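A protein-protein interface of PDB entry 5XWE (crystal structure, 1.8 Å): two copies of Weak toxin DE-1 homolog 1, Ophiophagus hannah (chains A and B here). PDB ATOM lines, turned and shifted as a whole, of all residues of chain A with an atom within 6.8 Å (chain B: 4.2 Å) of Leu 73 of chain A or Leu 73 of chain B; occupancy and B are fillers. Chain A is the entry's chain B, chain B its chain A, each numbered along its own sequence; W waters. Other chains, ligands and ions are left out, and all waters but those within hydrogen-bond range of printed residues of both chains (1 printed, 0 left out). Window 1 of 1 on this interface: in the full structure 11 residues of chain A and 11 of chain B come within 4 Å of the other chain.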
ATOM      1  N   TYR A  46     -10.041   7.932  29.115  1.00  0.00           N
ATOM      2  CA  TYR A  46     -10.716   6.985  29.987  1.00  0.00           C
ATOM      3  C   TYR A  46     -11.246   7.646  31.246  1.00  0.00           C
ATOM      4  O   TYR A  46     -10.745   8.666  31.716  1.00  0.00           O
ATOM      5  CB  TYR A  46      -9.813   5.807  30.380  1.00  0.00           C
ATOM      6  CG  TYR A  46      -8.823   6.095  31.481  1.00  0.00           C
ATOM      7  CD1 TYR A  46      -7.617   6.688  31.200  1.00  0.00           C
ATOM      8  CD2 TYR A  46      -9.090   5.765  32.795  1.00  0.00           C
ATOM      9  CE1 TYR A  46      -6.702   6.947  32.184  1.00  0.00           C
ATOM     10  CE2 TYR A  46      -8.175   6.022  33.791  1.00  0.00           C
ATOM     11  CZ  TYR A  46      -6.974   6.619  33.474  1.00  0.00           C
ATOM     12  OH  TYR A  46      -6.033   6.906  34.446  1.00  0.00           O
ATOM     13  N   ASN A  47     -12.272   7.010  31.792  1.00  0.00           N
ATOM     14  CA  ASN A  47     -12.875   7.382  33.063  1.00  0.00           C
ATOM     15  C   ASN A  47     -13.077   6.092  33.844  1.00  0.00           C
ATOM     16  O   ASN A  47     -13.901   5.259  33.461  1.00  0.00           O
ATOM     17  CB  ASN A  47     -14.188   8.127  32.845  1.00  0.00           C
ATOM     18  CG  ASN A  47     -14.828   8.558  34.136  1.00  0.00           C
ATOM     19  OD1 ASN A  47     -14.779   7.854  35.129  1.00  0.00           O
ATOM     20  ND2 ASN A  47     -15.409   9.741  34.137  1.00  0.00           N
ATOM     21  N   LEU A  48     -12.319   5.920  34.926  1.00  0.00           N
ATOM     22  CA  LEU A  48     -12.341   4.695  35.721  1.00  0.00           C
ATOM     23  C   LEU A  48     -12.869   4.953  37.127  1.00  0.00           C
ATOM     24  O   LEU A  48     -12.495   5.933  37.777  1.00  0.00           O
ATOM     25  CB  LEU A  48     -10.954   4.061  35.804  1.00  0.00           C
ATOM     26  CG  LEU A  48     -10.811   2.781  36.611  1.00  0.00           C
ATOM     27  CD1 LEU A  48      -9.798   1.907  35.932  1.00  0.00           C
ATOM     28  CD2 LEU A  48     -10.373   3.077  38.017  1.00  0.00           C
ATOM     29  N   PHE A  49     -13.714   4.037  37.592  1.00  0.00           N
ATOM     30  CA  PHE A  49     -14.354   4.078  38.898  1.00  0.00           C
ATOM     31  C   PHE A  49     -14.186   2.716  39.546  1.00  0.00           C
ATOM     32  O   PHE A  49     -14.395   1.688  38.895  1.00  0.00           O
ATOM     33  CB  PHE A  49     -15.833   4.438  38.754  1.00  0.00           C
ATOM     34  CG  PHE A  49     -16.591   4.495  40.042  1.00  0.00           C
ATOM     35  CD1 PHE A  49     -16.519   5.606  40.855  1.00  0.00           C
ATOM     36  CD2 PHE A  49     -17.411   3.451  40.421  1.00  0.00           C
ATOM     37  CE1 PHE A  49     -17.243   5.664  42.015  1.00  0.00           C
ATOM     38  CE2 PHE A  49     -18.129   3.503  41.587  1.00  0.00           C
ATOM     39  CZ  PHE A  49     -18.045   4.607  42.385  1.00  0.00           C
ATOM     40  N   CYS A  64      -6.537   3.803  27.723  1.00  0.00           N
ATOM     41  CA  CYS A  64      -7.608   2.958  28.231  1.00  0.00           C
ATOM     42  C   CYS A  64      -6.908   1.839  28.976  1.00  0.00           C
ATOM     43  O   CYS A  64      -6.324   0.952  28.342  1.00  0.00           O
ATOM     44  CB  CYS A  64      -8.474   2.420  27.099  1.00  0.00           C
ATOM     45  SG  CYS A  64      -9.901   1.499  27.634  1.00  0.00           S
ATOM     46  N   PRO A  65      -6.902   1.868  30.308  1.00  0.00           N
ATOM     47  CA  PRO A  65      -6.094   0.911  31.079  1.00  0.00           C
ATOM     48  C   PRO A  65      -6.570  -0.514  30.875  1.00  0.00           C
ATOM     49  O   PRO A  65      -7.736  -0.831  31.109  1.00  0.00           O
ATOM     50  CB  PRO A  65      -6.305   1.364  32.522  1.00  0.00           C
ATOM     51  CG  PRO A  65      -7.620   2.033  32.494  1.00  0.00           C
ATOM     52  CD  PRO A  65      -7.676   2.750  31.183  1.00  0.00           C
ATOM     53  N   LYS A  66      -5.647  -1.387  30.463  1.00  0.00           N
ATOM     54  CA  LYS A  66      -6.033  -2.755  30.154  1.00  0.00           C
ATOM     55  C   LYS A  66      -5.861  -3.702  31.323  1.00  0.00           C
ATOM     56  O   LYS A  66      -6.572  -4.708  31.405  1.00  0.00           O
ATOM     57  CB  LYS A  66      -5.228  -3.290  28.974  1.00  0.00           C
ATOM     58  CG  LYS A  66      -5.220  -2.379  27.769  1.00  0.00           C
ATOM     59  CD  LYS A  66      -6.529  -2.367  27.024  1.00  0.00           C
ATOM     60  CE  LYS A  66      -6.353  -1.634  25.712  1.00  0.00           C
ATOM     61  NZ  LYS A  66      -6.074  -0.171  25.908  1.00  0.00           N
ATOM     62  N   GLU A  68      -5.624  -2.602  34.754  1.00  0.00           N
ATOM     63  CA  GLU A  68      -5.927  -1.928  36.010  1.00  0.00           C
ATOM     64  C   GLU A  68      -7.328  -2.282  36.512  1.00  0.00           C
ATOM     65  O   GLU A  68      -8.276  -2.299  35.729  1.00  0.00           O
ATOM     66  CB  GLU A  68      -5.825  -0.430  35.822  1.00  0.00           C
ATOM     67  CG  GLU A  68      -6.227   0.361  37.032  1.00  0.00           C
ATOM     68  CD  GLU A  68      -5.810   1.809  36.931  1.00  0.00           C
ATOM     69  OE1 GLU A  68      -4.920   2.134  36.121  1.00  0.00           O
ATOM     70  OE2 GLU A  68      -6.342   2.628  37.698  1.00  0.00           O
ATOM     71  N   TYR A  70     -11.058  -2.187  38.082  1.00  0.00           N
ATOM     72  CA  TYR A  70     -12.111  -1.191  37.941  1.00  0.00           C
ATOM     73  C   TYR A  70     -13.441  -1.805  38.337  1.00  0.00           C
ATOM     74  O   TYR A  70     -13.602  -3.024  38.350  1.00  0.00           O
ATOM     75  CB  TYR A  70     -12.210  -0.669  36.504  1.00  0.00           C
ATOM     76  CG  TYR A  70     -12.658  -1.743  35.543  1.00  0.00           C
ATOM     77  CD1 TYR A  70     -11.743  -2.600  34.973  1.00  0.00           C
ATOM     78  CD2 TYR A  70     -13.998  -1.919  35.234  1.00  0.00           C
ATOM     79  CE1 TYR A  70     -12.143  -3.583  34.113  1.00  0.00           C
ATOM     80  CE2 TYR A  70     -14.403  -2.901  34.387  1.00  0.00           C
ATOM     81  CZ  TYR A  70     -13.472  -3.728  33.828  1.00  0.00           C
ATOM     82  OH  TYR A  70     -13.859  -4.723  32.978  1.00  0.00           O
ATOM     83  N   THR A  71     -14.404  -0.935  38.617  1.00  0.00           N
ATOM     84  CA  THR A  71     -15.807  -1.313  38.712  1.00  0.00           C
ATOM     85  C   THR A  71     -16.618  -0.845  37.514  1.00  0.00           C
ATOM     86  O   THR A  71     -17.383  -1.615  36.949  1.00  0.00           O
ATOM     87  CB  THR A  71     -16.403  -0.760  40.008  1.00  0.00           C
ATOM     88  OG1 THR A  71     -15.512  -1.050  41.087  1.00  0.00           O
ATOM     89  CG2 THR A  71     -17.749  -1.382  40.290  1.00  0.00           C
ATOM     90  N   ASN A  72     -16.458   0.407  37.111  1.00  0.00           N
ATOM     91  CA  ASN A  72     -16.975   0.925  35.854  1.00  0.00           C
ATOM     92  C   ASN A  72     -15.822   1.552  35.090  1.00  0.00           C
ATOM     93  O   ASN A  72     -15.099   2.381  35.640  1.00  0.00           O
ATOM     94  CB  ASN A  72     -18.056   1.974  36.080  1.00  0.00           C
ATOM     95  CG  ASN A  72     -19.104   1.518  37.024  1.00  0.00           C
ATOM     96  OD1 ASN A  72     -20.020   0.812  36.648  1.00  0.00           O
ATOM     97  ND2 ASN A  72     -19.003   1.944  38.258  1.00  0.00           N
ATOM     98  N   LEU A  73     -15.661   1.173  33.828  1.00  0.00           N
ATOM     99  CA  LEU A  73     -14.628   1.724  32.957  1.00  0.00           C
ATOM    100  C   LEU A  73     -15.265   2.220  31.664  1.00  0.00           C
ATOM    101  O   LEU A  73     -16.078   1.521  31.059  1.00  0.00           O
ATOM    102  CB  LEU A  73     -13.549   0.682  32.648  1.00  0.00           C
ATOM    103  CG  LEU A  73     -12.360   1.120  31.794  1.00  0.00           C
ATOM    104  CD1 LEU A  73     -11.616   2.255  32.450  1.00  0.00           C
ATOM    105  CD2 LEU A  73     -11.433  -0.035  31.499  1.00  0.00           C
ATOM    106  N   TYR A  74     -14.913   3.434  31.270  1.00  0.00           N
ATOM    107  CA  TYR A  74     -15.373   4.064  30.039  1.00  0.00           C
ATOM    108  C   TYR A  74     -14.164   4.578  29.282  1.00  0.00           C
ATOM    109  O   TYR A  74     -13.389   5.371  29.818  1.00  0.00           O
ATOM    110  CB  TYR A  74     -16.335   5.216  30.317  1.00  0.00           C
ATOM    111  CG  TYR A  74     -16.844   5.873  29.058  1.00  0.00           C
ATOM    112  CD1 TYR A  74     -17.704   5.193  28.198  1.00  0.00           C
ATOM    113  CD2 TYR A  74     -16.462   7.164  28.718  1.00  0.00           C
ATOM    114  CE1 TYR A  74     -18.180   5.789  27.040  1.00  0.00           C
ATOM    115  CE2 TYR A  74     -16.931   7.765  27.563  1.00  0.00           C
ATOM    116  CZ  TYR A  74     -17.789   7.068  26.726  1.00  0.00           C
ATOM    117  OH  TYR A  74     -18.258   7.644  25.584  1.00  0.00           O
ATOM    118  N   CYS A  75     -13.988   4.110  28.059  1.00  0.00           N
ATOM    119  CA  CYS A  75     -12.952   4.614  27.177  1.00  0.00           C
ATOM    120  C   CYS A  75     -13.596   5.140  25.905  1.00  0.00           C
ATOM    121  O   CYS A  75     -14.582   4.582  25.422  1.00  0.00           O
ATOM    122  CB  CYS A  75     -11.935   3.535  26.857  1.00  0.00           C
ATOM    123  SG  CYS A  75     -11.143   2.924  28.311  1.00  0.00           S
ATOM    124  N   CYS A  76     -13.045   6.215  25.370  1.00  0.00           N
ATOM    125  CA  CYS A  76     -13.655   6.874  24.233  1.00  0.00           C
ATOM    126  C   CYS A  76     -12.569   7.550  23.422  1.00  0.00           C
ATOM    127  O   CYS A  76     -11.509   7.883  23.944  1.00  0.00           O
ATOM    128  CB  CYS A  76     -14.693   7.879  24.693  1.00  0.00           C
ATOM    129  SG  CYS A  76     -14.018   8.973  25.926  1.00  0.00           S
ATOM    130  N   LYS A  77     -12.828   7.730  22.134  1.00  0.00           N
ATOM    131  CA  LYS A  77     -11.778   8.244  21.269  1.00  0.00           C
ATOM    132  C   LYS A  77     -12.154   9.580  20.643  1.00  0.00           C
ATOM    133  O   LYS A  77     -11.998   9.768  19.435  1.00  0.00           O
ATOM    134  CB  LYS A  77     -11.435   7.213  20.191  1.00  0.00           C
ATOM    135  CG  LYS A  77     -10.960   5.900  20.763  1.00  0.00           C
ATOM    136  CD  LYS A  77     -10.350   5.030  19.711  1.00  0.00           C
ATOM    137  CE  LYS A  77      -9.658   3.840  20.334  1.00  0.00           C
ATOM    138  NZ  LYS A  77      -9.386   2.751  19.353  1.00  0.00           N
ATOM    139  N   ASN B  47     -20.177  -2.774  26.722  1.00  0.00           N
ATOM    140  CA  ASN B  47     -20.925  -2.115  25.661  1.00  0.00           C
ATOM    141  C   ASN B  47     -19.922  -1.393  24.767  1.00  0.00           C
ATOM    142  O   ASN B  47     -19.280  -0.429  25.193  1.00  0.00           O
ATOM    143  CB  ASN B  47     -21.968  -1.164  26.249  1.00  0.00           C
ATOM    144  CG  ASN B  47     -22.826  -0.518  25.190  1.00  0.00           C
ATOM    145  OD1 ASN B  47     -22.347  -0.144  24.134  1.00  0.00           O
ATOM    146  ND2 ASN B  47     -24.114  -0.426  25.451  1.00  0.00           N
ATOM    147  N   LEU B  48     -19.777  -1.870  23.537  1.00  0.00           N
ATOM    148  CA  LEU B  48     -18.811  -1.335  22.581  1.00  0.00           C
ATOM    149  C   LEU B  48     -19.505  -0.676  21.393  1.00  0.00           C
ATOM    150  O   LEU B  48     -20.495  -1.190  20.865  1.00  0.00           O
ATOM    151  CB  LEU B  48     -17.854  -2.422  22.083  1.00  0.00           C
ATOM    152  CG  LEU B  48     -16.833  -2.030  21.023  1.00  0.00           C
ATOM    153  CD1 LEU B  48     -15.555  -2.778  21.276  1.00  0.00           C
ATOM    154  CD2 LEU B  48     -17.359  -2.378  19.659  1.00  0.00           C
ATOM    155  N   PRO B  65     -13.550  -6.362  26.275  1.00  0.00           N
ATOM    156  CA  PRO B  65     -12.568  -6.655  25.229  1.00  0.00           C
ATOM    157  C   PRO B  65     -11.333  -5.786  25.363  1.00  0.00           C
ATOM    158  O   PRO B  65     -11.424  -4.563  25.449  1.00  0.00           O
ATOM    159  CB  PRO B  65     -13.330  -6.346  23.940  1.00  0.00           C
ATOM    160  CG  PRO B  65     -14.358  -5.370  24.350  1.00  0.00           C
ATOM    161  CD  PRO B  65     -14.790  -5.818  25.715  1.00  0.00           C
ATOM    162  N   TYR B  70     -12.546  -0.020  19.008  1.00  0.00           N
ATOM    163  CA  TYR B  70     -13.762   0.594  19.498  1.00  0.00           C
ATOM    164  C   TYR B  70     -13.685   2.088  19.282  1.00  0.00           C
ATOM    165  O   TYR B  70     -12.608   2.653  19.104  1.00  0.00           O
ATOM    166  CB  TYR B  70     -13.956   0.313  20.984  1.00  0.00           C
ATOM    167  CG  TYR B  70     -12.895   0.956  21.851  1.00  0.00           C
ATOM    168  CD1 TYR B  70     -11.703   0.311  22.097  1.00  0.00           C
ATOM    169  CD2 TYR B  70     -13.080   2.212  22.409  1.00  0.00           C
ATOM    170  CE1 TYR B  70     -10.732   0.883  22.874  1.00  0.00           C
ATOM    171  CE2 TYR B  70     -12.108   2.791  23.184  1.00  0.00           C
ATOM    172  CZ  TYR B  70     -10.939   2.117  23.410  1.00  0.00           C
ATOM    173  OH  TYR B  70      -9.954   2.671  24.175  1.00  0.00           O
ATOM    174  N   ASN B  72     -16.386   3.974  21.413  1.00  0.00           N
ATOM    175  CA  ASN B  72     -16.731   4.087  22.822  1.00  0.00           C
ATOM    176  C   ASN B  72     -16.843   2.686  23.395  1.00  0.00           C
ATOM    177  O   ASN B  72     -17.528   1.835  22.826  1.00  0.00           O
ATOM    178  CB  ASN B  72     -18.040   4.838  23.034  1.00  0.00           C
ATOM    179  CG  ASN B  72     -18.105   6.100  22.258  1.00  0.00           C
ATOM    180  OD1 ASN B  72     -17.481   7.086  22.605  1.00  0.00           O
ATOM    181  ND2 ASN B  72     -18.899   6.099  21.224  1.00  0.00           N
ATOM    182  N   LEU B  73     -16.180   2.453  24.521  1.00  0.00           N
ATOM    183  CA  LEU B  73     -16.217   1.176  25.221  1.00  0.00           C
ATOM    184  C   LEU B  73     -16.628   1.410  26.669  1.00  0.00           C
ATOM    185  O   LEU B  73     -16.084   2.291  27.337  1.00  0.00           O
ATOM    186  CB  LEU B  73     -14.853   0.484  25.169  1.00  0.00           C
ATOM    187  CG  LEU B  73     -14.742  -0.899  25.800  1.00  0.00           C
ATOM    188  CD1 LEU B  73     -15.712  -1.846  25.133  1.00  0.00           C
ATOM    189  CD2 LEU B  73     -13.321  -1.411  25.703  1.00  0.00           C
ATOM    190  N   TYR B  74     -17.592   0.628  27.146  1.00  0.00           N
ATOM    191  CA  TYR B  74     -18.055   0.692  28.530  1.00  0.00           C
ATOM    192  C   TYR B  74     -18.028  -0.700  29.130  1.00  0.00           C
ATOM    193  O   TYR B  74     -18.692  -1.602  28.622  1.00  0.00           O
ATOM    194  CB  TYR B  74     -19.470   1.263  28.640  1.00  0.00           C
ATOM    195  CG  TYR B  74     -19.948   1.388  30.079  1.00  0.00           C
ATOM    196  CD1 TYR B  74     -19.366   2.308  30.956  1.00  0.00           C
ATOM    197  CD2 TYR B  74     -20.976   0.590  30.557  1.00  0.00           C
ATOM    198  CE1 TYR B  74     -19.806   2.430  32.260  1.00  0.00           C
ATOM    199  CE2 TYR B  74     -21.417   0.702  31.853  1.00  0.00           C
ATOM    200  CZ  TYR B  74     -20.829   1.620  32.704  1.00  0.00           C
ATOM    201  OH  TYR B  74     -21.279   1.715  33.990  1.00  0.00           O
ATOM    202  N   CYS B  75     -17.273  -0.870  30.205  1.00  0.00           N
ATOM    203  CA  CYS B  75     -17.264  -2.114  30.951  1.00  0.00           C
ATOM    204  C   CYS B  75     -17.662  -1.856  32.395  1.00  0.00           C
ATOM    205  O   CYS B  75     -17.302  -0.835  32.976  1.00  0.00           O
ATOM    206  CB  CYS B  75     -15.907  -2.771  30.902  1.00  0.00           C
ATOM    207  SG  CYS B  75     -15.415  -3.122  29.272  1.00  0.00           S
HETATM  208  O   HOH W   1     -10.269   1.517  17.439  1.00  0.00           O
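O of Tyr 74 of chain B is in hydrogen-bond range of N of Asn 47 of chain B (2.7 Å). N of Asn 47 of chain A sits at hydrogen-bond distance from O of Tyr 74 of chain A, at 2.8 Å. The side-chain sulfur (SG) of Cys 64 of chain A is disulfide-bonded to the side-chain sulfur (SG) of Cys 75 of chain A (2.0 Å). The backbone carbonyl oxygen (O) of Asn 72 of chain A lies within hydrogen-bond range of the backbone NH (N) of Phe 49 of chain A (2.9 Å). O of Cys 64 of chain A is in hydrogen-bond range of NZ of Lys 66 of chain A (2.7 Å).
Tyr 70 of chain A touches Cys 75 of chain B, and with the chains exchanged Cys 75 of chain A touches Tyr 70 of chain B. Leu 73 of chain B touches its own counterpart, Leu 73 of chain A. Leu 73 of chain A touches Tyr 74 of chain B, and with the chains exchanged Tyr 74 of chain A touches Leu 73 of chain B. Leu 73 of chain A touches Cys 75 of chain B, and with the chains exchanged Cys 75 of chain A touches Leu 73 of chain B.
Cys 75 of chain B touches Tyr 70 of chain A (CB to OH, 3.5 Å). CA of Asn 72 of chain A touches O of Cys 75 of chain B, 3.4 Å away. Leu 73 of chain B touches Leu 73 of chain A. Tyr 74 of chain B touches Leu 73 of chain A (CA to O, 3.3 Å). Tyr 74 of chain A touches Leu 73 of chain B (CA to O, 3.3 Å). Cys 75 of chain A touches Tyr 70 of chain B (CB to OH, 3.4 Å). Cys 75 of chain A touches Asn 72 of chain B (O to CA, 3.4 Å). CB of Cys 76 of chain A touches OD1 of Asn 72 of chain B, 3.6 Å away.
Water W1 lies within hydrogen-bond range of the side-chain amino group of Lys 77 of chain A (2.4 Å) and the backbone carbonyl oxygen of Tyr 70 of chain B (3.1 Å).
The side-chain amide oxygen of Asn 72 of chain B lies within hydrogen-bond range of the side-chain hydroxyl of Tyr 74 of chain A (3.1 Å). O of Cys 75 of chain B sits at hydrogen-bond distance from N of Leu 73 of chain A. OH of Tyr 74 of chain B lies within hydrogen-bond range of OD1 of Asn 72 of chain A. O of Tyr 70 of chain B sits at hydrogen-bond distance from NZ of Lys 77 of chain A (3.2 Å). The side-chain hydroxyl (OH) of Tyr 70 of chain B lies close to the side-chain sulfur (SG) of Cys 64 of chain A (3.7 Å). N of Leu 73 of chain B lies within hydrogen-bond range of O of Cys 75 of chain A.
Of the 16 printed residues of chain A, 8 touch a printed residue of chain B. Hydrophobic or aromatic side chains of chain A within 4 Å of the printed part of chain B: Tyr 70 and Tyr 74. Among the printed residues, 14 pairs touch across the chains. Among the printed residues, no Asp or Glu carboxylate lies within 4 Å of a Lys or Arg side-chain nitrogen of the other chain.
Tyr 46 of chain A touches none of the printed residues of chain B. Of the printed residues of chain B, Asn 72 of chain A touches Tyr 74 (3.1 Å) and Cys 75 (3.4 Å). Leu 73 of chain A touches just these residues of chain B: Leu 73, Tyr 74 and Cys 75. Printed residues of chain B within 4 Å of Tyr 74 of chain A: Asn 72 (3.1 Å) and Leu 73 (3.3 Å). Of the printed residues of chain B, Cys 75 of chain A touches Tyr 70, Asn 72 and Leu 73. Of the printed residues of chain B, Cys 76 of chain A touches Asn 72 (3.6 Å). Pro 65 of chain B touches none of the printed residues of chain A. Of chain A, only Leu 73 (3.8 Å), Tyr 74 (3.3 Å) and Cys 75 (2.8 Å) come within 4 Å of Leu 73 of chain B. Printed residues of chain A within 4 Å of Tyr 74 of chain B: Asn 72 and Leu 73. The nearest printed residue of chain B that does not touch Leu 73 of chain A is Asn 47 of chain B (7.0 Å).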
